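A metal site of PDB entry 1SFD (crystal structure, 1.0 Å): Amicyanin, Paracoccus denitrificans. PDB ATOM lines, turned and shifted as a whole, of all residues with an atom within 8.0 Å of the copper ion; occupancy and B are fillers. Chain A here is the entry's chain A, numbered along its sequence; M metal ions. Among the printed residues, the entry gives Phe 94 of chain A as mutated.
ND1 of His 53 is bound to the copper ion. The copper ion is bound by ND1 of His 95. SG of Cys 92 is bound to the copper ion (2.2 Å). The copper ion has three donor atoms within binding distance. Slightly farther from the copper ion lies the side-chain sulfur (SD) of Met 98 (2.8 Å).
O of Pro 52 touches the copper ion (3.8 Å). Of the 20 residues printed, 5 come within 4 Å of the copper ion. The nearest printed residue that does not touch the copper ion is Phe 94 (4.4 Å).
The backbone NH of Met 72 lies within hydrogen-bond range of the backbone carbonyl oxygen of His 53. ND1 of His 95 sits close to SD of Met 98 (3.7 Å). N of Asn 54 lies close to SG of Cys 92, 3.5 Å away. OE2 of Glu 49 lies within hydrogen-bond range of NE2 of His 53 (2.8 Å). SD of Met 51 sits at hydrogen-bond distance from NE2 of His 95, at 3.6 Å. The side-chain hydroxyl of Tyr 30 sits at hydrogen-bond distance from the backbone NH of Cys 92, at 3.1 Å. SG of Cys 92 lies close to N of Phe 94 (3.6 Å). SD of Met 98 lies close to ND1 of His 53.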
ATOM      1  N   ILE A  25      13.902  16.531 -20.798  1.00  0.00           N
ATOM      2  CA  ILE A  25      14.715  16.643 -22.023  1.00  0.00           C
ATOM      3  C   ILE A  25      16.123  16.310 -21.650  1.00  0.00           C
ATOM      4  O   ILE A  25      16.725  16.987 -20.760  1.00  0.00           O
ATOM      5  CB  ILE A  25      14.603  18.041 -22.671  1.00  0.00           C
ATOM      6  CG1 ILE A  25      13.205  18.604 -22.649  1.00  0.00           C
ATOM      7  CG2 ILE A  25      15.171  17.954 -24.093  1.00  0.00           C
ATOM      8  CD1 ILE A  25      13.100  20.026 -23.175  1.00  0.00           C
ATOM      9  N   MET A  28      19.728  14.834 -25.833  1.00  0.00           N
ATOM     10  CA  MET A  28      19.228  15.223 -27.156  1.00  0.00           C
ATOM     11  C   MET A  28      17.914  14.531 -27.502  1.00  0.00           C
ATOM     12  O   MET A  28      17.615  14.367 -28.693  1.00  0.00           O
ATOM     13  CB  MET A  28      20.268  15.012 -28.244  1.00  0.00           C
ATOM     14  CG  MET A  28      21.604  15.662 -27.952  1.00  0.00           C
ATOM     15  SD  MET A  28      21.588  17.449 -27.855  1.00  0.00           S
ATOM     16  CE  MET A  28      21.188  17.887 -29.539  1.00  0.00           C
ATOM     17  N   LYS A  29      17.088  14.203 -26.502  1.00  0.00           N
ATOM     18  CA  LYS A  29      15.819  13.587 -26.715  1.00  0.00           C
ATOM     19  C   LYS A  29      14.768  14.079 -25.726  1.00  0.00           C
ATOM     20  O   LYS A  29      15.132  14.425 -24.594  1.00  0.00           O
ATOM     21  CB  LYS A  29      15.893  12.056 -26.589  1.00  0.00           C
ATOM     22  CG  LYS A  29      16.813  11.400 -27.583  1.00  0.00           C
ATOM     23  CD  LYS A  29      16.958   9.914 -27.385  1.00  0.00           C
ATOM     24  CE  LYS A  29      17.792   9.248 -28.417  1.00  0.00           C
ATOM     25  NZ  LYS A  29      18.930  10.013 -28.962  1.00  0.00           N
ATOM     26  N   TYR A  30      13.528  14.100 -26.167  1.00  0.00           N
ATOM     27  CA  TYR A  30      12.412  14.195 -25.229  1.00  0.00           C
ATOM     28  C   TYR A  30      12.215  12.781 -24.651  1.00  0.00           C
ATOM     29  O   TYR A  30      12.090  11.821 -25.383  1.00  0.00           O
ATOM     30  CB  TYR A  30      11.173  14.669 -25.934  1.00  0.00           C
ATOM     31  CG  TYR A  30      11.300  16.031 -26.561  1.00  0.00           C
ATOM     32  CD1 TYR A  30      11.373  17.172 -25.803  1.00  0.00           C
ATOM     33  CD2 TYR A  30      11.409  16.154 -27.953  1.00  0.00           C
ATOM     34  CE1 TYR A  30      11.523  18.437 -26.369  1.00  0.00           C
ATOM     35  CE2 TYR A  30      11.536  17.385 -28.535  1.00  0.00           C
ATOM     36  CZ  TYR A  30      11.595  18.526 -27.757  1.00  0.00           C
ATOM     37  OH  TYR A  30      11.680  19.722 -28.415  1.00  0.00           O
ATOM     38  N   ASN A  47      14.280  20.944 -19.155  1.00  0.00           N
ATOM     39  CA  ASN A  47      15.560  20.642 -19.736  1.00  0.00           C
ATOM     40  C   ASN A  47      16.502  20.165 -18.596  1.00  0.00           C
ATOM     41  O   ASN A  47      16.735  20.934 -17.656  1.00  0.00           O
ATOM     42  CB  ASN A  47      16.165  21.864 -20.442  1.00  0.00           C
ATOM     43  CG  ASN A  47      17.432  21.497 -21.173  1.00  0.00           C
ATOM     44  OD1 ASN A  47      17.827  20.302 -21.187  1.00  0.00           O
ATOM     45  ND2 ASN A  47      18.064  22.488 -21.801  1.00  0.00           N
ATOM     46  N   GLU A  49      19.728  19.176 -19.121  1.00  0.00           N
ATOM     47  CA  GLU A  49      21.118  19.209 -19.546  1.00  0.00           C
ATOM     48  C   GLU A  49      21.549  20.595 -19.990  1.00  0.00           C
ATOM     49  O   GLU A  49      20.736  21.521 -20.155  1.00  0.00           O
ATOM     50  CB  GLU A  49      21.378  18.159 -20.609  1.00  0.00           C
ATOM     51  CG  GLU A  49      20.690  18.379 -21.945  1.00  0.00           C
ATOM     52  CD  GLU A  49      20.919  17.273 -22.932  1.00  0.00           C
ATOM     53  OE1 GLU A  49      21.542  16.229 -22.502  1.00  0.00           O
ATOM     54  OE2 GLU A  49      20.453  17.334 -24.083  1.00  0.00           O
ATOM     55  N   MET A  51      22.996  21.627 -22.809  1.00  0.00           N
ATOM     56  CA  MET A  51      22.603  22.006 -24.170  1.00  0.00           C
ATOM     57  C   MET A  51      21.234  22.649 -24.138  1.00  0.00           C
ATOM     58  O   MET A  51      20.293  22.029 -23.631  1.00  0.00           O
ATOM     59  CB  MET A  51      22.525  20.748 -25.055  1.00  0.00           C
ATOM     60  CG  MET A  51      21.982  21.062 -26.418  1.00  0.00           C
ATOM     61  SD  MET A  51      22.948  22.160 -27.458  1.00  0.00           S
ATOM     62  CE  MET A  51      24.296  21.073 -27.912  1.00  0.00           C
ATOM     63  N   PRO A  52      21.050  23.854 -24.706  1.00  0.00           N
ATOM     64  CA  PRO A  52      19.719  24.427 -24.690  1.00  0.00           C
ATOM     65  C   PRO A  52      18.765  23.683 -25.606  1.00  0.00           C
ATOM     66  O   PRO A  52      19.169  23.133 -26.625  1.00  0.00           O
ATOM     67  CB  PRO A  52      19.959  25.857 -25.220  1.00  0.00           C
ATOM     68  CG  PRO A  52      21.392  26.124 -24.890  1.00  0.00           C
ATOM     69  CD  PRO A  52      22.065  24.803 -25.140  1.00  0.00           C
ATOM     70  N   HIS A  53      17.494  23.699 -25.232  1.00  0.00           N
ATOM     71  CA  HIS A  53      16.408  23.094 -26.001  1.00  0.00           C
ATOM     72  C   HIS A  53      15.153  23.949 -25.881  1.00  0.00           C
ATOM     73  O   HIS A  53      15.080  24.824 -25.014  1.00  0.00           O
ATOM     74  CB  HIS A  53      16.096  21.670 -25.529  1.00  0.00           C
ATOM     75  CG  HIS A  53      17.224  20.709 -25.612  1.00  0.00           C
ATOM     76  ND1 HIS A  53      17.713  20.241 -26.829  1.00  0.00           N
ATOM     77  CD2 HIS A  53      17.919  20.098 -24.604  1.00  0.00           C
ATOM     78  CE1 HIS A  53      18.702  19.392 -26.531  1.00  0.00           C
ATOM     79  NE2 HIS A  53      18.848  19.296 -25.210  1.00  0.00           N
ATOM     80  N   ASN A  54      14.155  23.670 -26.703  1.00  0.00           N
ATOM     81  CA  ASN A  54      12.824  24.234 -26.508  1.00  0.00           C
ATOM     82  C   ASN A  54      11.796  23.204 -26.951  1.00  0.00           C
ATOM     83  O   ASN A  54      12.144  22.065 -27.219  1.00  0.00           O
ATOM     84  CB  ASN A  54      12.648  25.587 -27.192  1.00  0.00           C
ATOM     85  CG  ASN A  54      12.472  25.467 -28.690  1.00  0.00           C
ATOM     86  OD1 ASN A  54      12.787  24.440 -29.257  1.00  0.00           O
ATOM     87  ND2 ASN A  54      11.952  26.577 -29.245  1.00  0.00           N
ATOM     88  N   VAL A  55      10.529  23.624 -27.024  1.00  0.00           N
ATOM     89  CA  VAL A  55       9.474  22.926 -27.731  1.00  0.00           C
ATOM     90  C   VAL A  55       8.874  23.882 -28.741  1.00  0.00           C
ATOM     91  O   VAL A  55       8.725  25.068 -28.465  1.00  0.00           O
ATOM     92  CB  VAL A  55       8.383  22.338 -26.807  1.00  0.00           C
ATOM     93  CG1 VAL A  55       9.034  21.271 -25.904  1.00  0.00           C
ATOM     94  CG2 VAL A  55       7.686  23.379 -26.022  1.00  0.00           C
ATOM     95  N   MET A  72      15.338  27.097 -23.364  1.00  0.00           N
ATOM     96  CA  MET A  72      15.419  26.571 -22.001  1.00  0.00           C
ATOM     97  C   MET A  72      16.837  26.127 -21.703  1.00  0.00           C
ATOM     98  O   MET A  72      17.372  25.265 -22.432  1.00  0.00           O
ATOM     99  CB  MET A  72      14.486  25.367 -21.874  1.00  0.00           C
ATOM    100  CG  MET A  72      13.037  25.684 -22.216  1.00  0.00           C
ATOM    101  SD  MET A  72      12.021  24.228 -22.564  1.00  0.00           S
ATOM    102  CE  MET A  72      11.930  23.594 -20.948  1.00  0.00           C
ATOM    103  N   HIS A  91       8.778  19.756 -32.065  1.00  0.00           N
ATOM    104  CA  HIS A  91      10.184  19.468 -32.198  1.00  0.00           C
ATOM    105  C   HIS A  91      10.981  20.543 -31.456  1.00  0.00           C
ATOM    106  O   HIS A  91      10.394  21.518 -30.963  1.00  0.00           O
ATOM    107  CB  HIS A  91      10.595  19.373 -33.680  1.00  0.00           C
ATOM    108  CG  HIS A  91      10.519  20.694 -34.415  1.00  0.00           C
ATOM    109  ND1 HIS A  91       9.331  21.145 -35.000  1.00  0.00           N
ATOM    110  CD2 HIS A  91      11.451  21.648 -34.666  1.00  0.00           C
ATOM    111  CE1 HIS A  91       9.592  22.338 -35.574  1.00  0.00           C
ATOM    112  NE2 HIS A  91      10.845  22.659 -35.393  1.00  0.00           N
ATOM    113  N   CYS A  92      12.281  20.387 -31.432  1.00  0.00           N
ATOM    114  CA  CYS A  92      13.149  21.382 -30.859  1.00  0.00           C
ATOM    115  C   CYS A  92      13.637  22.302 -31.971  1.00  0.00           C
ATOM    116  O   CYS A  92      14.202  21.828 -32.945  1.00  0.00           O
ATOM    117  CB  CYS A  92      14.351  20.678 -30.168  1.00  0.00           C
ATOM    118  SG  CYS A  92      15.509  21.904 -29.458  1.00  0.00           S
ATOM    119  N   THR A  93      13.429  23.614 -31.839  1.00  0.00           N
ATOM    120  CA  THR A  93      13.873  24.547 -32.857  1.00  0.00           C
ATOM    121  C   THR A  93      15.343  24.354 -33.169  1.00  0.00           C
ATOM    122  O   THR A  93      15.781  24.419 -34.316  1.00  0.00           O
ATOM    123  CB  THR A  93      13.627  25.993 -32.397  1.00  0.00           C
ATOM    124  OG1 THR A  93      12.260  26.148 -32.129  1.00  0.00           O
ATOM    125  CG2 THR A  93      14.059  26.972 -33.481  1.00  0.00           C
ATOM    126  N   PHE A  94      16.141  24.191 -32.100  1.00  0.00           N
ATOM    127  CA  PHE A  94      17.585  24.109 -32.304  1.00  0.00           C
ATOM    128  C   PHE A  94      17.994  22.813 -32.968  1.00  0.00           C
ATOM    129  O   PHE A  94      18.995  22.748 -33.679  1.00  0.00           O
ATOM    130  CB  PHE A  94      18.305  24.235 -30.956  1.00  0.00           C
ATOM    131  CG  PHE A  94      17.870  25.442 -30.165  1.00  0.00           C
ATOM    132  CD1 PHE A  94      17.048  25.380 -29.069  1.00  0.00           C
ATOM    133  CD2 PHE A  94      18.305  26.690 -30.570  1.00  0.00           C
ATOM    134  CE1 PHE A  94      16.618  26.487 -28.382  1.00  0.00           C
ATOM    135  CE2 PHE A  94      17.889  27.808 -29.853  1.00  0.00           C
ATOM    136  CZ  PHE A  94      17.048  27.706 -28.780  1.00  0.00           C
ATOM    137  N   HIS A  95      17.225  21.752 -32.655  1.00  0.00           N
ATOM    138  CA  HIS A  95      17.556  20.386 -33.050  1.00  0.00           C
ATOM    139  C   HIS A  95      16.319  19.718 -33.593  1.00  0.00           C
ATOM    140  O   HIS A  95      15.672  18.919 -32.892  1.00  0.00           O
ATOM    141  CB  HIS A  95      18.099  19.608 -31.828  1.00  0.00           C
ATOM    142  CG  HIS A  95      19.118  20.383 -31.048  1.00  0.00           C
ATOM    143  ND1 HIS A  95      18.897  20.799 -29.742  1.00  0.00           N
ATOM    144  CD2 HIS A  95      20.348  20.854 -31.378  1.00  0.00           C
ATOM    145  CE1 HIS A  95      19.945  21.476 -29.313  1.00  0.00           C
ATOM    146  NE2 HIS A  95      20.867  21.536 -30.305  1.00  0.00           N
ATOM    147  N   PRO A  96      15.926  20.024 -34.825  1.00  0.00           N
ATOM    148  CA  PRO A  96      14.594  19.574 -35.283  1.00  0.00           C
ATOM    149  C   PRO A  96      14.407  18.048 -35.350  1.00  0.00           C
ATOM    150  O   PRO A  96      13.304  17.558 -35.297  1.00  0.00           O
ATOM    151  CB  PRO A  96      14.431  20.242 -36.651  1.00  0.00           C
ATOM    152  CG  PRO A  96      15.255  21.498 -36.535  1.00  0.00           C
ATOM    153  CD  PRO A  96      16.485  21.042 -35.746  1.00  0.00           C
ATOM    154  N   PHE A  97      15.519  17.306 -35.417  1.00  0.00           N
ATOM    155  CA  PHE A  97      15.448  15.859 -35.365  1.00  0.00           C
ATOM    156  C   PHE A  97      14.906  15.361 -34.017  1.00  0.00           C
ATOM    157  O   PHE A  97      14.489  14.194 -33.967  1.00  0.00           O
ATOM    158  CB  PHE A  97      16.836  15.246 -35.673  1.00  0.00           C
ATOM    159  CG  PHE A  97      17.948  15.714 -34.728  1.00  0.00           C
ATOM    160  CD1 PHE A  97      18.161  15.084 -33.497  1.00  0.00           C
ATOM    161  CD2 PHE A  97      18.757  16.780 -35.094  1.00  0.00           C
ATOM    162  CE1 PHE A  97      19.144  15.560 -32.652  1.00  0.00           C
ATOM    163  CE2 PHE A  97      19.738  17.221 -34.235  1.00  0.00           C
ATOM    164  CZ  PHE A  97      19.945  16.620 -33.020  1.00  0.00           C
ATOM    165  N   MET A  98      14.943  16.188 -32.980  1.00  0.00           N
ATOM    166  CA  MET A  98      14.342  15.875 -31.677  1.00  0.00           C
ATOM    167  C   MET A  98      12.862  16.127 -31.765  1.00  0.00           C
ATOM    168  O   MET A  98      12.467  17.314 -31.930  1.00  0.00           O
ATOM    169  CB  MET A  98      14.836  16.842 -30.576  1.00  0.00           C
ATOM    170  CG  MET A  98      16.281  16.709 -30.237  1.00  0.00           C
ATOM    171  SD  MET A  98      16.792  17.857 -28.952  1.00  0.00           S
ATOM    172  CE  MET A  98      15.721  17.494 -27.588  1.00  0.00           C
HETATM  173 CU    CU M   1      17.151  20.623 -28.687  1.00  0.00          CU
